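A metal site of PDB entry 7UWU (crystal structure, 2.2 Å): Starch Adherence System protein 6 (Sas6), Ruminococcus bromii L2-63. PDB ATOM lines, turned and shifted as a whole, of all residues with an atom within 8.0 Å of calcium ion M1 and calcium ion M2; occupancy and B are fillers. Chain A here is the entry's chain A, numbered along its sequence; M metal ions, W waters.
Calcium ion M1 is bound by OD2 of Asp 528, OD1 of Asp 510, O of Ser 507, OD1 of Asp 530, water W1, OE2 of Glu 525 and OE1 of Glu 525.
Calcium ion M1 has seven donor atoms within binding distance.
The side-chain carboxylate (OE1) of Glu 525 binds calcium ion M2.
The side-chain carboxylate (OD1) of Asp 528 binds calcium ion M2 (2.4 Å).
Calcium ion M2 is bound by OD2 of Asp 530 (2.4 Å).
O of Gly 498 is bound to calcium ion M2.
OG of Ser 497 is bound to calcium ion M2 (2.5 Å).
The backbone carbonyl oxygen (O) of Glu 525 binds calcium ion M2, at 2.5 Å.
OD1 of Asp 530 is bound to calcium ion M2 (2.7 Å).
Water W1 bridges the side-chain carboxylate of Asp 510 (2.7 Å) and the backbone carbonyl oxygen of Ile 529 (2.8 Å).
N of Asp 530 lies within hydrogen-bond range of O of Gly 354.
O of Asp 528 is in hydrogen-bond range of N of Gly 354 (3.2 Å).
OG of Ser 523 is in hydrogen-bond range of N of Glu 525 (3.1 Å).
N of Asn 531 is in hydrogen-bond range of OG of Ser 507.
N of Ser 497 lies close to O of Lys 526 (3.4 Å).
The backbone NH (N) of Gly 498 sits at hydrogen-bond distance from the side-chain hydroxyl (OG1) of Thr 355 (3.2 Å).
OD2 of Asp 528 sits close to OE1 of Gln 511, 3.0 Å away.
OE2 of Glu 525 lies close to N of Gln 511, at 2.9 Å.
The nearest printed residue that does not touch calcium ion M1 is Gln 511 (4.3 Å).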
ATOM      1  N   PRO A 250      21.088 -25.664  18.429  1.00  0.00           N
ATOM      2  CA  PRO A 250      22.469 -25.965  18.869  1.00  0.00           C
ATOM      3  C   PRO A 250      22.758 -25.650  20.324  1.00  0.00           C
ATOM      4  O   PRO A 250      23.526 -26.390  20.958  1.00  0.00           O
ATOM      5  CB  PRO A 250      23.327 -25.092  17.931  1.00  0.00           C
ATOM      6  CG  PRO A 250      22.524 -25.022  16.673  1.00  0.00           C
ATOM      7  CD  PRO A 250      21.064 -25.022  17.095  1.00  0.00           C
ATOM      8  N   GLY A 353      30.644 -17.938   8.889  1.00  0.00           N
ATOM      9  CA  GLY A 353      29.629 -18.968   8.815  1.00  0.00           C
ATOM     10  C   GLY A 353      28.743 -18.844   7.581  1.00  0.00           C
ATOM     11  O   GLY A 353      28.712 -17.825   6.894  1.00  0.00           O
ATOM     12  N   GLY A 354      28.013 -19.916   7.337  1.00  0.00           N
ATOM     13  CA  GLY A 354      27.123 -19.969   6.189  1.00  0.00           C
ATOM     14  C   GLY A 354      26.625 -21.383   6.006  1.00  0.00           C
ATOM     15  O   GLY A 354      27.076 -22.324   6.663  1.00  0.00           O
ATOM     16  N   THR A 355      25.648 -21.512   5.098  1.00  0.00           N
ATOM     17  CA  THR A 355      25.077 -22.810   4.769  1.00  0.00           C
ATOM     18  C   THR A 355      25.227 -23.051   3.271  1.00  0.00           C
ATOM     19  O   THR A 355      24.787 -22.220   2.471  1.00  0.00           O
ATOM     20  CB  THR A 355      23.603 -22.898   5.190  1.00  0.00           C
ATOM     21  OG1 THR A 355      23.509 -22.710   6.606  1.00  0.00           O
ATOM     22  CG2 THR A 355      23.034 -24.259   4.846  1.00  0.00           C
ATOM     23  N   LEU A 492      17.182 -21.429   9.395  1.00  0.00           N
ATOM     24  CA  LEU A 492      17.265 -20.396  10.414  1.00  0.00           C
ATOM     25  C   LEU A 492      18.732 -20.159  10.748  1.00  0.00           C
ATOM     26  O   LEU A 492      19.536 -21.096  10.762  1.00  0.00           O
ATOM     27  CB  LEU A 492      16.507 -20.773  11.687  1.00  0.00           C
ATOM     28  CG  LEU A 492      14.983 -20.920  11.620  1.00  0.00           C
ATOM     29  CD1 LEU A 492      14.405 -21.234  12.993  1.00  0.00           C
ATOM     30  CD2 LEU A 492      14.345 -19.671  11.045  1.00  0.00           C
ATOM     31  N   THR A 493      19.075 -18.912  11.026  1.00  0.00           N
ATOM     32  CA  THR A 493      20.443 -18.553  11.383  1.00  0.00           C
ATOM     33  C   THR A 493      20.428 -17.771  12.695  1.00  0.00           C
ATOM     34  O   THR A 493      19.373 -17.383  13.204  1.00  0.00           O
ATOM     35  CB  THR A 493      21.114 -17.712  10.282  1.00  0.00           C
ATOM     36  OG1 THR A 493      20.804 -16.321  10.507  1.00  0.00           O
ATOM     37  CG2 THR A 493      20.659 -18.141   8.869  1.00  0.00           C
ATOM     38  N   TYR A 494      21.620 -17.536  13.229  1.00  0.00           N
ATOM     39  CA  TYR A 494      21.821 -16.526  14.261  1.00  0.00           C
ATOM     40  C   TYR A 494      22.765 -15.452  13.757  1.00  0.00           C
ATOM     41  O   TYR A 494      23.716 -15.047  14.441  1.00  0.00           O
ATOM     42  CB  TYR A 494      22.340 -17.145  15.556  1.00  0.00           C
ATOM     43  CG  TYR A 494      22.103 -16.298  16.787  1.00  0.00           C
ATOM     44  CD1 TYR A 494      21.463 -15.065  16.681  1.00  0.00           C
ATOM     45  CD2 TYR A 494      22.512 -16.720  18.045  1.00  0.00           C
ATOM     46  CE1 TYR A 494      21.246 -14.279  17.788  1.00  0.00           C
ATOM     47  CE2 TYR A 494      22.288 -15.935  19.165  1.00  0.00           C
ATOM     48  CZ  TYR A 494      21.654 -14.714  19.029  1.00  0.00           C
ATOM     49  OH  TYR A 494      21.422 -13.914  20.116  1.00  0.00           O
ATOM     50  N   THR A 496      24.678 -15.705  10.626  1.00  0.00           N
ATOM     51  CA  THR A 496      25.342 -16.192   9.418  1.00  0.00           C
ATOM     52  C   THR A 496      25.086 -17.696   9.189  1.00  0.00           C
ATOM     53  O   THR A 496      24.260 -18.070   8.355  1.00  0.00           O
ATOM     54  CB  THR A 496      26.836 -15.934   9.484  1.00  0.00           C
ATOM     55  OG1 THR A 496      27.335 -16.403  10.747  1.00  0.00           O
ATOM     56  CG2 THR A 496      27.126 -14.437   9.343  1.00  0.00           C
ATOM     57  N   SER A 497      25.809 -18.533   9.932  1.00  0.00           N
ATOM     58  CA  SER A 497      25.663 -19.978   9.856  1.00  0.00           C
ATOM     59  C   SER A 497      24.230 -20.419  10.182  1.00  0.00           C
ATOM     60  O   SER A 497      23.502 -19.767  10.939  1.00  0.00           O
ATOM     61  CB  SER A 497      26.635 -20.639  10.839  1.00  0.00           C
ATOM     62  OG  SER A 497      26.779 -22.004  10.586  1.00  0.00           O
ATOM     63  N   GLY A 498      23.820 -21.540   9.604  1.00  0.00           N
ATOM     64  CA  GLY A 498      22.549 -22.123   9.989  1.00  0.00           C
ATOM     65  C   GLY A 498      22.560 -22.610  11.438  1.00  0.00           C
ATOM     66  O   GLY A 498      23.598 -22.839  12.048  1.00  0.00           O
ATOM     67  N   MET A 499      21.342 -22.763  11.986  1.00  0.00           N
ATOM     68  CA  MET A 499      21.121 -23.332  13.307  1.00  0.00           C
ATOM     69  C   MET A 499      20.109 -24.451  13.288  1.00  0.00           C
ATOM     70  O   MET A 499      20.248 -25.425  14.022  1.00  0.00           O
ATOM     71  CB  MET A 499      20.642 -22.268  14.310  1.00  0.00           C
ATOM     72  CG  MET A 499      21.541 -21.046  14.407  1.00  0.00           C
ATOM     73  SD  MET A 499      22.922 -21.333  15.494  1.00  0.00           S
ATOM     74  CE  MET A 499      22.256 -20.794  17.092  1.00  0.00           C
ATOM     75  N   ASP A 500      19.073 -24.335  12.460  1.00  0.00           N
ATOM     76  CA  ASP A 500      17.976 -25.284  12.428  1.00  0.00           C
ATOM     77  C   ASP A 500      17.401 -25.235  11.024  1.00  0.00           C
ATOM     78  O   ASP A 500      17.401 -24.180  10.380  1.00  0.00           O
ATOM     79  CB  ASP A 500      16.922 -24.933  13.499  1.00  0.00           C
ATOM     80  CG  ASP A 500      15.983 -26.103  13.845  1.00  0.00           C
ATOM     81  OD1 ASP A 500      15.911 -27.080  13.074  1.00  0.00           O
ATOM     82  OD2 ASP A 500      15.296 -26.015  14.892  1.00  0.00           O
ATOM     83  N   ASP A 505      18.349 -30.960   8.954  1.00  0.00           N
ATOM     84  CA  ASP A 505      19.605 -31.516   8.402  1.00  0.00           C
ATOM     85  C   ASP A 505      20.657 -31.733   9.492  1.00  0.00           C
ATOM     86  O   ASP A 505      20.845 -30.847  10.338  1.00  0.00           O
ATOM     87  CB  ASP A 505      20.175 -30.587   7.311  1.00  0.00           C
ATOM     88  CG  ASP A 505      21.398 -31.186   6.604  1.00  0.00           C
ATOM     89  OD1 ASP A 505      22.506 -31.144   7.209  1.00  0.00           O
ATOM     90  OD2 ASP A 505      21.245 -31.669   5.453  1.00  0.00           O
ATOM     91  N   PRO A 506      21.367 -32.887   9.507  1.00  0.00           N
ATOM     92  CA  PRO A 506      22.334 -33.134  10.592  1.00  0.00           C
ATOM     93  C   PRO A 506      23.481 -32.144  10.629  1.00  0.00           C
ATOM     94  O   PRO A 506      24.124 -32.019  11.678  1.00  0.00           O
ATOM     95  CB  PRO A 506      22.845 -34.555  10.301  1.00  0.00           C
ATOM     96  CG  PRO A 506      22.602 -34.759   8.874  1.00  0.00           C
ATOM     97  CD  PRO A 506      21.326 -33.998   8.553  1.00  0.00           C
ATOM     98  N   SER A 507      23.757 -31.427   9.540  1.00  0.00           N
ATOM     99  CA  SER A 507      24.859 -30.474   9.630  1.00  0.00           C
ATOM    100  C   SER A 507      24.498 -29.291  10.529  1.00  0.00           C
ATOM    101  O   SER A 507      25.382 -28.485  10.868  1.00  0.00           O
ATOM    102  CB  SER A 507      25.311 -30.037   8.221  1.00  0.00           C
ATOM    103  OG  SER A 507      24.579 -28.975   7.618  1.00  0.00           O
ATOM    104  N   MET A 508      23.259 -29.228  11.015  1.00  0.00           N
ATOM    105  CA  MET A 508      22.881 -28.200  11.974  1.00  0.00           C
ATOM    106  C   MET A 508      23.434 -28.480  13.372  1.00  0.00           C
ATOM    107  O   MET A 508      23.447 -27.594  14.238  1.00  0.00           O
ATOM    108  CB  MET A 508      21.358 -28.100  12.048  1.00  0.00           C
ATOM    109  CG  MET A 508      20.721 -27.491  10.815  1.00  0.00           C
ATOM    110  SD  MET A 508      21.347 -25.881  10.303  1.00  0.00           S
ATOM    111  CE  MET A 508      22.087 -26.212   8.702  1.00  0.00           C
ATOM    112  N   LEU A 509      23.876 -29.722  13.612  1.00  0.00           N
ATOM    113  CA  LEU A 509      24.286 -30.156  14.940  1.00  0.00           C
ATOM    114  C   LEU A 509      25.593 -30.926  14.920  1.00  0.00           C
ATOM    115  O   LEU A 509      26.012 -31.447  15.966  1.00  0.00           O
ATOM    116  CB  LEU A 509      23.165 -31.018  15.590  1.00  0.00           C
ATOM    117  CG  LEU A 509      21.819 -30.317  15.843  1.00  0.00           C
ATOM    118  CD1 LEU A 509      20.754 -31.313  16.354  1.00  0.00           C
ATOM    119  CD2 LEU A 509      22.002 -29.177  16.820  1.00  0.00           C
ATOM    120  N   ASP A 510      26.259 -31.031  13.759  1.00  0.00           N
ATOM    121  CA  ASP A 510      27.507 -31.782  13.674  1.00  0.00           C
ATOM    122  C   ASP A 510      28.618 -31.140  14.494  1.00  0.00           C
ATOM    123  O   ASP A 510      29.606 -31.819  14.798  1.00  0.00           O
ATOM    124  CB  ASP A 510      27.945 -31.971  12.215  1.00  0.00           C
ATOM    125  CG  ASP A 510      28.278 -30.660  11.506  1.00  0.00           C
ATOM    126  OD1 ASP A 510      27.712 -29.592  11.855  1.00  0.00           O
ATOM    127  OD2 ASP A 510      29.116 -30.689  10.577  1.00  0.00           O
ATOM    128  N   GLN A 511      28.473 -29.877  14.883  1.00  0.00           N
ATOM    129  CA  GLN A 511      29.439 -29.212  15.747  1.00  0.00           C
ATOM    130  C   GLN A 511      28.764 -28.495  16.914  1.00  0.00           C
ATOM    131  O   GLN A 511      29.352 -27.583  17.504  1.00  0.00           O
ATOM    132  CB  GLN A 511      30.312 -28.267  14.926  1.00  0.00           C
ATOM    133  CG  GLN A 511      30.761 -28.883  13.586  1.00  0.00           C
ATOM    134  CD  GLN A 511      31.969 -28.177  12.965  1.00  0.00           C
ATOM    135  OE1 GLN A 511      31.836 -27.150  12.303  1.00  0.00           O
ATOM    136  NE2 GLN A 511      33.151 -28.742  13.171  1.00  0.00           N
ATOM    137  N   ALA A 512      27.547 -28.915  17.297  1.00  0.00           N
ATOM    138  CA  ALA A 512      26.746 -28.142  18.255  1.00  0.00           C
ATOM    139  C   ALA A 512      27.426 -27.963  19.610  1.00  0.00           C
ATOM    140  O   ALA A 512      27.226 -26.930  20.268  1.00  0.00           O
ATOM    141  CB  ALA A 512      25.380 -28.794  18.431  1.00  0.00           C
ATOM    142  N   SER A 523      27.460 -21.911  21.339  1.00  0.00           N
ATOM    143  CA  SER A 523      27.785 -22.961  20.400  1.00  0.00           C
ATOM    144  C   SER A 523      28.494 -22.420  19.156  1.00  0.00           C
ATOM    145  O   SER A 523      28.172 -21.366  18.627  1.00  0.00           O
ATOM    146  CB  SER A 523      26.528 -23.708  19.948  1.00  0.00           C
ATOM    147  OG  SER A 523      26.850 -24.616  18.922  1.00  0.00           O
ATOM    148  N   HIS A 524      29.437 -23.222  18.670  1.00  0.00           N
ATOM    149  CA  HIS A 524      30.126 -22.926  17.418  1.00  0.00           C
ATOM    150  C   HIS A 524      29.180 -22.917  16.212  1.00  0.00           C
ATOM    151  O   HIS A 524      29.477 -22.234  15.223  1.00  0.00           O
ATOM    152  CB  HIS A 524      31.281 -23.933  17.268  1.00  0.00           C
ATOM    153  CG  HIS A 524      32.167 -23.697  16.078  1.00  0.00           C
ATOM    154  ND1 HIS A 524      32.819 -22.503  15.859  1.00  0.00           N
ATOM    155  CD2 HIS A 524      32.561 -24.520  15.072  1.00  0.00           C
ATOM    156  CE1 HIS A 524      33.544 -22.591  14.759  1.00  0.00           C
ATOM    157  NE2 HIS A 524      33.399 -23.808  14.270  1.00  0.00           N
ATOM    158  N   GLU A 525      28.030 -23.615  16.271  1.00  0.00           N
ATOM    159  CA  GLU A 525      27.147 -23.681  15.110  1.00  0.00           C
ATOM    160  C   GLU A 525      26.708 -22.314  14.611  1.00  0.00           C
ATOM    161  O   GLU A 525      26.192 -22.220  13.491  1.00  0.00           O
ATOM    162  CB  GLU A 525      25.893 -24.528  15.409  1.00  0.00           C
ATOM    163  CG  GLU A 525      26.095 -26.046  15.315  1.00  0.00           C
ATOM    164  CD  GLU A 525      26.341 -26.573  13.897  1.00  0.00           C
ATOM    165  OE1 GLU A 525      26.062 -25.848  12.918  1.00  0.00           O
ATOM    166  OE2 GLU A 525      26.820 -27.723  13.766  1.00  0.00           O
ATOM    167  N   LYS A 526      26.879 -21.241  15.393  1.00  0.00           N
ATOM    168  CA  LYS A 526      26.564 -19.905  14.917  1.00  0.00           C
ATOM    169  C   LYS A 526      27.517 -19.432  13.826  1.00  0.00           C
ATOM    170  O   LYS A 526      27.157 -18.510  13.076  1.00  0.00           O
ATOM    171  CB  LYS A 526      26.616 -18.899  16.076  1.00  0.00           C
ATOM    172  CG  LYS A 526      25.730 -19.269  17.242  1.00  0.00           C
ATOM    173  CD  LYS A 526      25.619 -18.127  18.230  1.00  0.00           C
ATOM    174  CE  LYS A 526      26.610 -18.299  19.391  1.00  0.00           C
ATOM    175  NZ  LYS A 526      26.617 -17.125  20.313  1.00  0.00           N
ATOM    176  N   GLU A 527      28.704 -20.025  13.724  1.00  0.00           N
ATOM    177  CA  GLU A 527      29.760 -19.465  12.889  1.00  0.00           C
ATOM    178  C   GLU A 527      30.385 -20.487  11.945  1.00  0.00           C
ATOM    179  O   GLU A 527      31.271 -20.115  11.172  1.00  0.00           O
ATOM    180  CB  GLU A 527      30.867 -18.842  13.767  1.00  0.00           C
ATOM    181  CG  GLU A 527      31.544 -19.870  14.733  1.00  0.00           C
ATOM    182  CD  GLU A 527      32.747 -19.338  15.543  1.00  0.00           C
ATOM    183  OE1 GLU A 527      33.239 -18.205  15.321  1.00  0.00           O
ATOM    184  OE2 GLU A 527      33.191 -20.074  16.434  1.00  0.00           O
ATOM    185  N   ASP A 528      29.979 -21.756  11.987  1.00  0.00           N
ATOM    186  CA  ASP A 528      30.605 -22.762  11.132  1.00  0.00           C
ATOM    187  C   ASP A 528      29.919 -22.806   9.766  1.00  0.00           C
ATOM    188  O   ASP A 528      29.011 -22.033   9.463  1.00  0.00           O
ATOM    189  CB  ASP A 528      30.583 -24.136  11.806  1.00  0.00           C
ATOM    190  CG  ASP A 528      29.180 -24.729  11.909  1.00  0.00           C
ATOM    191  OD1 ASP A 528      28.203 -23.946  11.865  1.00  0.00           O
ATOM    192  OD2 ASP A 528      29.058 -25.965  12.049  1.00  0.00           O
ATOM    193  N   ILE A 529      30.383 -23.747   8.937  1.00  0.00           N
ATOM    194  CA  ILE A 529      29.910 -23.910   7.563  1.00  0.00           C
ATOM    195  C   ILE A 529      29.066 -25.172   7.519  1.00  0.00           C
ATOM    196  O   ILE A 529      29.562 -26.273   7.762  1.00  0.00           O
ATOM    197  CB  ILE A 529      31.090 -23.989   6.576  1.00  0.00           C
ATOM    198  CG1 ILE A 529      31.875 -22.689   6.598  1.00  0.00           C
ATOM    199  CG2 ILE A 529      30.620 -24.304   5.154  1.00  0.00           C
ATOM    200  CD1 ILE A 529      32.576 -22.395   5.296  1.00  0.00           C
ATOM    201  N   ASP A 530      27.787 -25.004   7.212  1.00  0.00           N
ATOM    202  CA  ASP A 530      26.854 -26.115   7.097  1.00  0.00           C
ATOM    203  C   ASP A 530      26.754 -26.536   5.639  1.00  0.00           C
ATOM    204  O   ASP A 530      27.088 -25.781   4.723  1.00  0.00           O
ATOM    205  CB  ASP A 530      25.476 -25.716   7.652  1.00  0.00           C
ATOM    206  CG  ASP A 530      25.543 -25.293   9.132  1.00  0.00           C
ATOM    207  OD1 ASP A 530      26.347 -25.871   9.874  1.00  0.00           O
ATOM    208  OD2 ASP A 530      24.791 -24.379   9.548  1.00  0.00           O
ATOM    209  N   ASN A 531      26.302 -27.757   5.422  1.00  0.00           N
ATOM    210  CA  ASN A 531      26.198 -28.285   4.060  1.00  0.00           C
ATOM    211  C   ASN A 531      25.000 -29.209   4.024  1.00  0.00           C
ATOM    212  O   ASN A 531      25.006 -30.245   4.696  1.00  0.00           O
ATOM    213  CB  ASN A 531      27.483 -29.004   3.660  1.00  0.00           C
ATOM    214  CG  ASN A 531      27.268 -29.927   2.481  1.00  0.00           C
ATOM    215  OD1 ASN A 531      26.564 -29.574   1.548  1.00  0.00           O
ATOM    216  ND2 ASN A 531      27.881 -31.115   2.518  1.00  0.00           N
HETATM  217 CA    CA M   1      27.397 -27.366  11.415  1.00  0.00          CA
HETATM  218 CA    CA M   2      25.772 -23.956  11.742  1.00  0.00          CA
HETATM  219  O   HOH W   1      28.674 -28.267   9.534  1.00  0.00           O
